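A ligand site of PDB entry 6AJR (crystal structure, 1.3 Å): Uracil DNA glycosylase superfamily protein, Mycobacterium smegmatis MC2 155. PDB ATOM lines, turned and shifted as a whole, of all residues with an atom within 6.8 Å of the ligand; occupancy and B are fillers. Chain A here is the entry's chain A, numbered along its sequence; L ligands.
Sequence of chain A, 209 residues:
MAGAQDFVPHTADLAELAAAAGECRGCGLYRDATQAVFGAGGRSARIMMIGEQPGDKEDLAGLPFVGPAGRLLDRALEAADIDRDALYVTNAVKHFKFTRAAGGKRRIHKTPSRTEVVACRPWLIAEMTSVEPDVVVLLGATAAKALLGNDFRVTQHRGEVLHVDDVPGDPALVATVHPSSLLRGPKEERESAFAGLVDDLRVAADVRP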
ATOM      1  N   GLY A   3     -25.224 -17.937 -18.416  1.00  0.00           N
ATOM      2  CA  GLY A   3     -24.909 -16.525 -18.633  1.00  0.00           C
ATOM      3  C   GLY A   3     -24.970 -16.116 -20.091  1.00  0.00           C
ATOM      4  O   GLY A   3     -25.960 -16.352 -20.794  1.00  0.00           O
ATOM      5  N   ALA A   4     -23.889 -15.505 -20.576  1.00  0.00           N
ATOM      6  CA  ALA A   4     -23.845 -15.010 -21.948  1.00  0.00           C
ATOM      7  C   ALA A   4     -23.639 -16.107 -22.992  1.00  0.00           C
ATOM      8  O   ALA A   4     -23.695 -15.801 -24.183  1.00  0.00           O
ATOM      9  CB  ALA A   4     -22.726 -13.980 -22.122  1.00  0.00           C
ATOM     10  N   PHE A   7     -25.471 -16.457 -26.242  1.00  0.00           N
ATOM     11  CA  PHE A   7     -25.457 -15.275 -27.086  1.00  0.00           C
ATOM     12  C   PHE A   7     -24.170 -15.097 -27.888  1.00  0.00           C
ATOM     13  O   PHE A   7     -24.116 -14.237 -28.765  1.00  0.00           O
ATOM     14  CB  PHE A   7     -25.721 -14.023 -26.227  1.00  0.00           C
ATOM     15  CG  PHE A   7     -27.070 -14.042 -25.551  1.00  0.00           C
ATOM     16  CD1 PHE A   7     -28.200 -13.674 -26.238  1.00  0.00           C
ATOM     17  CD2 PHE A   7     -27.188 -14.426 -24.227  1.00  0.00           C
ATOM     18  CE1 PHE A   7     -29.454 -13.696 -25.625  1.00  0.00           C
ATOM     19  CE2 PHE A   7     -28.433 -14.448 -23.603  1.00  0.00           C
ATOM     20  CZ  PHE A   7     -29.570 -14.094 -24.304  1.00  0.00           C
ATOM     21  N   ALA A  21     -22.666  -9.031 -29.113  1.00  0.00           N
ATOM     22  CA  ALA A  21     -22.734  -8.575 -27.726  1.00  0.00           C
ATOM     23  C   ALA A  21     -23.806  -7.512 -27.531  1.00  0.00           C
ATOM     24  O   ALA A  21     -24.381  -7.413 -26.441  1.00  0.00           O
ATOM     25  CB  ALA A  21     -21.362  -8.070 -27.273  1.00  0.00           C
ATOM     26  N   GLY A  22     -24.099  -6.726 -28.566  1.00  0.00           N
ATOM     27  CA  GLY A  22     -25.167  -5.744 -28.458  1.00  0.00           C
ATOM     28  C   GLY A  22     -26.517  -6.379 -28.180  1.00  0.00           C
ATOM     29  O   GLY A  22     -27.391  -5.722 -27.601  1.00  0.00           O
ATOM     30  N   GLU A  23     -26.698  -7.638 -28.567  1.00  0.00           N
ATOM     31  CA  GLU A  23     -27.943  -8.375 -28.361  1.00  0.00           C
ATOM     32  C   GLU A  23     -27.887  -9.273 -27.138  1.00  0.00           C
ATOM     33  O   GLU A  23     -28.847  -9.997 -26.879  1.00  0.00           O
ATOM     34  CB  GLU A  23     -28.245  -9.213 -29.601  1.00  0.00           C
ATOM     35  CG  GLU A  23     -28.424  -8.376 -30.847  1.00  0.00           C
ATOM     36  CD  GLU A  23     -29.407  -7.243 -30.636  1.00  0.00           C
ATOM     37  OE1 GLU A  23     -29.020  -6.069 -30.821  1.00  0.00           O
ATOM     38  OE2 GLU A  23     -30.571  -7.538 -30.279  1.00  0.00           O
ATOM     39  N   CYS A  24     -26.804  -9.245 -26.384  1.00  0.00           N
ATOM     40  CA  CYS A  24     -26.685 -10.142 -25.244  1.00  0.00           C
ATOM     41  C   CYS A  24     -27.681  -9.775 -24.156  1.00  0.00           C
ATOM     42  O   CYS A  24     -27.900  -8.602 -23.851  1.00  0.00           O
ATOM     43  CB  CYS A  24     -25.265 -10.065 -24.681  1.00  0.00           C
ATOM     44  SG  CYS A  24     -24.949 -11.283 -23.392  1.00  0.00           S
ATOM     45  N   ARG A  25     -28.292 -10.800 -23.553  1.00  0.00           N
ATOM     46  CA  ARG A  25     -29.112 -10.650 -22.353  1.00  0.00           C
ATOM     47  C   ARG A  25     -28.612 -11.572 -21.236  1.00  0.00           C
ATOM     48  O   ARG A  25     -29.406 -12.004 -20.392  1.00  0.00           O
ATOM     49  CB  ARG A  25     -30.590 -10.919 -22.659  1.00  0.00           C
ATOM     50  CG  ARG A  25     -31.166 -10.005 -23.756  1.00  0.00           C
ATOM     51  CD  ARG A  25     -32.685 -10.149 -23.925  1.00  0.00           C
ATOM     52  NE  ARG A  25     -33.115 -11.547 -23.992  1.00  0.00           N
ATOM     53  CZ  ARG A  25     -33.056 -12.307 -25.088  1.00  0.00           C
ATOM     54  NH1 ARG A  25     -32.574 -11.814 -26.223  1.00  0.00           N
ATOM     55  NH2 ARG A  25     -33.450 -13.571 -25.036  1.00  0.00           N
ATOM     56  N   GLY A  26     -27.314 -11.870 -21.237  1.00  0.00           N
ATOM     57  CA  GLY A  26     -26.757 -12.861 -20.329  1.00  0.00           C
ATOM     58  C   GLY A  26     -26.865 -12.512 -18.851  1.00  0.00           C
ATOM     59  O   GLY A  26     -26.752 -13.405 -17.997  1.00  0.00           O
ATOM     60  N   CYS A  27     -27.002 -11.227 -18.523  1.00  0.00           N
ATOM     61  CA  CYS A  27     -27.291 -10.785 -17.160  1.00  0.00           C
ATOM     62  C   CYS A  27     -28.257  -9.609 -17.273  1.00  0.00           C
ATOM     63  O   CYS A  27     -28.803  -9.324 -18.347  1.00  0.00           O
ATOM     64  CB  CYS A  27     -26.014 -10.514 -16.351  1.00  0.00           C
ATOM     65  SG  CYS A  27     -25.137  -8.981 -16.739  1.00  0.00           S
ATOM     66  N   GLY A  28     -28.491  -8.894 -16.175  1.00  0.00           N
ATOM     67  CA  GLY A  28     -29.445  -7.798 -16.271  1.00  0.00           C
ATOM     68  C   GLY A  28     -28.860  -6.489 -16.759  1.00  0.00           C
ATOM     69  O   GLY A  28     -29.619  -5.538 -16.977  1.00  0.00           O
ATOM     70  N   LEU A  29     -27.542  -6.408 -16.951  1.00  0.00           N
ATOM     71  CA  LEU A  29     -26.905  -5.115 -17.166  1.00  0.00           C
ATOM     72  C   LEU A  29     -27.242  -4.488 -18.508  1.00  0.00           C
ATOM     73  O   LEU A  29     -27.143  -3.269 -18.649  1.00  0.00           O
ATOM     74  CB  LEU A  29     -25.394  -5.226 -16.952  1.00  0.00           C
ATOM     75  CG  LEU A  29     -25.012  -5.577 -15.511  1.00  0.00           C
ATOM     76  CD1 LEU A  29     -23.500  -5.701 -15.410  1.00  0.00           C
ATOM     77  CD2 LEU A  29     -25.560  -4.568 -14.516  1.00  0.00           C
ATOM     78  N   TYR A  30     -27.655  -5.279 -19.502  1.00  0.00           N
ATOM     79  CA  TYR A  30     -28.010  -4.706 -20.790  1.00  0.00           C
ATOM     80  C   TYR A  30     -29.190  -3.735 -20.689  1.00  0.00           C
ATOM     81  O   TYR A  30     -29.337  -2.867 -21.560  1.00  0.00           O
ATOM     82  CB  TYR A  30     -28.347  -5.807 -21.802  1.00  0.00           C
ATOM     83  CG  TYR A  30     -29.697  -6.442 -21.571  1.00  0.00           C
ATOM     84  CD1 TYR A  30     -29.861  -7.466 -20.643  1.00  0.00           C
ATOM     85  CD2 TYR A  30     -30.824  -6.001 -22.261  1.00  0.00           C
ATOM     86  CE1 TYR A  30     -31.096  -8.052 -20.419  1.00  0.00           C
ATOM     87  CE2 TYR A  30     -32.067  -6.567 -22.039  1.00  0.00           C
ATOM     88  CZ  TYR A  30     -32.194  -7.591 -21.116  1.00  0.00           C
ATOM     89  OH  TYR A  30     -33.423  -8.161 -20.896  1.00  0.00           O
ATOM     90  N   ARG A  31     -30.037  -3.862 -19.661  1.00  0.00           N
ATOM     91  CA  ARG A  31     -31.299  -3.124 -19.655  1.00  0.00           C
ATOM     92  C   ARG A  31     -31.086  -1.621 -19.569  1.00  0.00           C
ATOM     93  O   ARG A  31     -31.664  -0.856 -20.345  1.00  0.00           O
ATOM     94  CB  ARG A  31     -32.197  -3.617 -18.515  1.00  0.00           C
ATOM     95  CG  ARG A  31     -32.637  -5.060 -18.685  1.00  0.00           C
ATOM     96  CD  ARG A  31     -33.743  -5.450 -17.701  1.00  0.00           C
ATOM     97  NE  ARG A  31     -33.721  -6.888 -17.449  1.00  0.00           N
ATOM     98  CZ  ARG A  31     -33.497  -7.427 -16.254  1.00  0.00           C
ATOM     99  NH1 ARG A  31     -33.485  -8.745 -16.097  1.00  0.00           N
ATOM    100  NH2 ARG A  31     -33.297  -6.646 -15.196  1.00  0.00           N
ATOM    101  N   ALA A  36     -23.653  -2.238 -25.524  1.00  0.00           N
ATOM    102  CA  ALA A  36     -22.480  -2.999 -25.124  1.00  0.00           C
ATOM    103  C   ALA A  36     -21.223  -2.278 -25.604  1.00  0.00           C
ATOM    104  O   ALA A  36     -21.213  -1.631 -26.666  1.00  0.00           O
ATOM    105  CB  ALA A  36     -22.530  -4.414 -25.727  1.00  0.00           C
ATOM    106  N   ALA A  92     -14.000  -6.797 -18.315  1.00  0.00           N
ATOM    107  CA  ALA A  92     -14.576  -8.051 -17.844  1.00  0.00           C
ATOM    108  C   ALA A  92     -16.080  -8.113 -18.062  1.00  0.00           C
ATOM    109  O   ALA A  92     -16.617  -9.189 -18.329  1.00  0.00           O
ATOM    110  CB  ALA A  92     -14.246  -8.241 -16.377  1.00  0.00           C
ATOM    111  N   VAL A  93     -16.762  -6.986 -17.945  1.00  0.00           N
ATOM    112  CA  VAL A  93     -18.204  -6.892 -18.163  1.00  0.00           C
ATOM    113  C   VAL A  93     -18.425  -5.840 -19.243  1.00  0.00           C
ATOM    114  O   VAL A  93     -17.689  -4.848 -19.308  1.00  0.00           O
ATOM    115  CB  VAL A  93     -18.858  -6.509 -16.818  1.00  0.00           C
ATOM    116  CG1 VAL A  93     -20.256  -6.018 -16.974  1.00  0.00           C
ATOM    117  CG2 VAL A  93     -18.833  -7.736 -15.914  1.00  0.00           C
ATOM    118  N   LYS A  94     -19.411  -6.072 -20.126  1.00  0.00           N
ATOM    119  CA  LYS A  94     -19.546  -5.288 -21.354  1.00  0.00           C
ATOM    120  C   LYS A  94     -20.632  -4.231 -21.288  1.00  0.00           C
ATOM    121  O   LYS A  94     -20.726  -3.405 -22.205  1.00  0.00           O
ATOM    122  CB  LYS A  94     -19.801  -6.192 -22.579  1.00  0.00           C
ATOM    123  CG  LYS A  94     -18.769  -7.297 -22.833  1.00  0.00           C
ATOM    124  CD  LYS A  94     -17.365  -6.768 -22.961  1.00  0.00           C
ATOM    125  CE  LYS A  94     -16.445  -7.733 -23.764  1.00  0.00           C
ATOM    126  NZ  LYS A  94     -15.506  -8.421 -22.843  1.00  0.00           N
ATOM    127  N   HIS A  95     -21.458  -4.218 -20.251  1.00  0.00           N
ATOM    128  CA  HIS A  95     -22.464  -3.191 -20.086  1.00  0.00           C
ATOM    129  C   HIS A  95     -22.209  -2.428 -18.785  1.00  0.00           C
ATOM    130  O   HIS A  95     -21.945  -3.037 -17.754  1.00  0.00           O
ATOM    131  CB  HIS A  95     -23.874  -3.778 -20.064  1.00  0.00           C
ATOM    132  CG  HIS A  95     -24.404  -4.138 -21.419  1.00  0.00           C
ATOM    133  ND1 HIS A  95     -24.505  -5.448 -21.857  1.00  0.00           N
ATOM    134  CD2 HIS A  95     -24.895  -3.369 -22.421  1.00  0.00           C
ATOM    135  CE1 HIS A  95     -25.026  -5.456 -23.082  1.00  0.00           C
ATOM    136  NE2 HIS A  95     -25.271  -4.215 -23.438  1.00  0.00           N
ATOM    137  N   PHE A  96     -22.305  -1.109 -18.850  1.00  0.00           N
ATOM    138  CA  PHE A  96     -22.091  -0.212 -17.721  1.00  0.00           C
ATOM    139  C   PHE A  96     -23.169  -0.427 -16.660  1.00  0.00           C
ATOM    140  O   PHE A  96     -24.365  -0.372 -16.969  1.00  0.00           O
ATOM    141  CB  PHE A  96     -22.212   1.198 -18.299  1.00  0.00           C
ATOM    142  CG  PHE A  96     -22.020   2.338 -17.330  1.00  0.00           C
ATOM    143  CD1 PHE A  96     -21.113   2.315 -16.282  1.00  0.00           C
ATOM    144  CD2 PHE A  96     -22.730   3.517 -17.554  1.00  0.00           C
ATOM    145  CE1 PHE A  96     -20.933   3.447 -15.471  1.00  0.00           C
ATOM    146  CE2 PHE A  96     -22.571   4.619 -16.762  1.00  0.00           C
ATOM    147  CZ  PHE A  96     -21.670   4.602 -15.718  1.00  0.00           C
ATOM    148  N   GLU A 116     -22.359 -11.484 -12.223  1.00  0.00           N
ATOM    149  CA  GLU A 116     -22.313 -10.772 -13.487  1.00  0.00           C
ATOM    150  C   GLU A 116     -20.993 -11.005 -14.221  1.00  0.00           C
ATOM    151  O   GLU A 116     -20.974 -11.181 -15.445  1.00  0.00           O
ATOM    152  CB  GLU A 116     -22.573  -9.277 -13.260  1.00  0.00           C
ATOM    153  CG  GLU A 116     -24.035  -9.001 -12.955  1.00  0.00           C
ATOM    154  CD  GLU A 116     -24.283  -7.713 -12.176  1.00  0.00           C
ATOM    155  OE1 GLU A 116     -23.356  -7.140 -11.572  1.00  0.00           O
ATOM    156  OE2 GLU A 116     -25.446  -7.290 -12.180  1.00  0.00           O
ATOM    157  N   VAL A 118     -19.050 -13.699 -14.019  1.00  0.00           N
ATOM    158  CA  VAL A 118     -19.066 -15.044 -14.559  1.00  0.00           C
ATOM    159  C   VAL A 118     -20.032 -15.128 -15.743  1.00  0.00           C
ATOM    160  O   VAL A 118     -19.744 -15.796 -16.748  1.00  0.00           O
ATOM    161  CB  VAL A 118     -19.400 -16.052 -13.446  1.00  0.00           C
ATOM    162  CG1 VAL A 118     -19.706 -17.449 -14.025  1.00  0.00           C
ATOM    163  CG2 VAL A 118     -18.243 -16.120 -12.438  1.00  0.00           C
ATOM    164  N   ALA A 119     -21.168 -14.417 -15.649  1.00  0.00           N
ATOM    165  CA  ALA A 119     -22.132 -14.403 -16.751  1.00  0.00           C
ATOM    166  C   ALA A 119     -21.513 -13.844 -18.033  1.00  0.00           C
ATOM    167  O   ALA A 119     -21.778 -14.341 -19.130  1.00  0.00           O
ATOM    168  CB  ALA A 119     -23.375 -13.586 -16.368  1.00  0.00           C
ATOM    169  N   CYS A 120     -20.683 -12.798 -17.909  1.00  0.00           N
ATOM    170  CA  CYS A 120     -20.145 -12.109 -19.084  1.00  0.00           C
ATOM    171  C   CYS A 120     -18.845 -12.734 -19.583  1.00  0.00           C
ATOM    172  O   CYS A 120     -18.432 -12.477 -20.722  1.00  0.00           O
ATOM    173  CB  CYS A 120     -19.905 -10.636 -18.758  1.00  0.00           C
ATOM    174  SG  CYS A 120     -19.888  -9.553 -20.224  1.00  0.00           S
ATOM    175  N   ARG A 121     -18.209 -13.545 -18.772  1.00  0.00           N
ATOM    176  CA  ARG A 121     -16.919 -14.122 -19.112  1.00  0.00           C
ATOM    177  C   ARG A 121     -16.868 -14.863 -20.445  1.00  0.00           C
ATOM    178  O   ARG A 121     -15.803 -14.871 -21.082  1.00  0.00           O
ATOM    179  CB  ARG A 121     -16.429 -15.020 -17.968  1.00  0.00           C
ATOM    180  CG  ARG A 121     -14.953 -15.389 -18.069  1.00  0.00           C
ATOM    181  CD  ARG A 121     -14.435 -15.935 -16.772  1.00  0.00           C
ATOM    182  NE  ARG A 121     -15.227 -17.076 -16.339  1.00  0.00           N
ATOM    183  CZ  ARG A 121     -15.152 -17.614 -15.126  1.00  0.00           C
ATOM    184  NH1 ARG A 121     -14.313 -17.097 -14.238  1.00  0.00           N
ATOM    185  NH2 ARG A 121     -15.910 -18.641 -14.788  1.00  0.00           N
ATOM    186  N   PRO A 122     -17.940 -15.494 -20.924  1.00  0.00           N
ATOM    187  CA  PRO A 122     -17.869 -16.085 -22.276  1.00  0.00           C
ATOM    188  C   PRO A 122     -17.465 -15.105 -23.364  1.00  0.00           C
ATOM    189  O   PRO A 122     -16.833 -15.522 -24.342  1.00  0.00           O
ATOM    190  CB  PRO A 122     -19.276 -16.667 -22.482  1.00  0.00           C
ATOM    191  CG  PRO A 122     -19.709 -17.029 -21.091  1.00  0.00           C
ATOM    192  CD  PRO A 122     -19.182 -15.903 -20.226  1.00  0.00           C
ATOM    193  N   TRP A 123     -17.770 -13.822 -23.229  1.00  0.00           N
ATOM    194  CA  TRP A 123     -17.280 -12.843 -24.205  1.00  0.00           C
ATOM    195  C   TRP A 123     -15.773 -12.698 -24.111  1.00  0.00           C
ATOM    196  O   TRP A 123     -15.088 -12.642 -25.147  1.00  0.00           O
ATOM    197  CB  TRP A 123     -17.961 -11.487 -24.024  1.00  0.00           C
ATOM    198  CG  TRP A 123     -19.406 -11.499 -24.360  1.00  0.00           C
ATOM    199  CD1 TRP A 123     -20.461 -11.327 -23.500  1.00  0.00           C
ATOM    200  CD2 TRP A 123     -19.982 -11.717 -25.657  1.00  0.00           C
ATOM    201  NE1 TRP A 123     -21.650 -11.427 -24.180  1.00  0.00           N
ATOM    202  CE2 TRP A 123     -21.392 -11.678 -25.499  1.00  0.00           C
ATOM    203  CE3 TRP A 123     -19.462 -11.951 -26.933  1.00  0.00           C
ATOM    204  CZ2 TRP A 123     -22.266 -11.848 -26.575  1.00  0.00           C
ATOM    205  CZ3 TRP A 123     -20.320 -12.128 -27.994  1.00  0.00           C
ATOM    206  CH2 TRP A 123     -21.708 -12.082 -27.809  1.00  0.00           C
HETATM  207 FE1  LIG L   1     -24.028  -7.308 -20.948  1.00  0.00          FE
HETATM  208 FE2  LIG L   1     -22.103  -9.101 -20.381  1.00  0.00          FE
HETATM  209 FE3  LIG L   1     -24.358  -9.851 -21.601  1.00  0.00          FE
HETATM  210 FE4  LIG L   1     -24.423  -9.058 -18.972  1.00  0.00          FE
HETATM  211  S1  LIG L   1     -23.401 -10.913 -19.821  1.00  0.00           S
HETATM  212  S2  LIG L   1     -25.944  -8.511 -20.624  1.00  0.00           S
HETATM  213  S3  LIG L   1     -22.842  -7.380 -19.018  1.00  0.00           S
HETATM  214  S4  LIG L   1     -22.768  -8.487 -22.477  1.00  0.00           S
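The backbone NH (N) of His 95 sits close to a sulfur (S3) of the ligand, 3.7 Å away.
FE1 of the ligand is bound by ND1 of His 95 (2.1 Å).
An iron atom (FE2) of the ligand is bound by the side-chain sulfur (SG) of Cys 120, at 2.3 Å.
A sulfur (S2) of the ligand lies close to the backbone NH (N) of Cys 27, 3.6 Å away.
The side-chain sulfur (SG) of Cys 27 is bound to an iron atom (FE4) of the ligand, at 2.3 Å.
SG of Cys 24 binds FE3 of the ligand (2.4 Å).
NE1 of Trp 123 lies close to S4 of the ligand, 3.6 Å away.
S2 of the ligand sits close to N of Gly 26, at 3.7 Å.
A ring nitrogen (NE2) of His 95 sits at hydrogen-bond distance from the backbone NH of Ala 36 (3.3 Å).
The side-chain sulfur (SG) of Cys 120 sits close to the backbone NH (N) of Lys 94 (3.5 Å).
The side-chain sulfur (SG) of Cys 120 sits close to the backbone carbonyl oxygen (O) of Ala 92.
SG of Cys 27 sits close to N of Leu 29 (3.5 Å).
The side-chain sulfur (SG) of Cys 24 lies close to the indole nitrogen (NE1) of Trp 123 (3.4 Å).
SG of Cys 24 lies close to N of Gly 26, at 3.3 Å.
The backbone carbonyl oxygen (O) of Ala 119 sits at hydrogen-bond distance from the backbone NH (N) of Ala 4.
Residues that only touch the ligand: Val 93, Lys 94, Tyr 30, Ala 119, Ala 4 and Leu 29.
Of the 27 residues printed, 12 come within 4 Å of the ligand.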
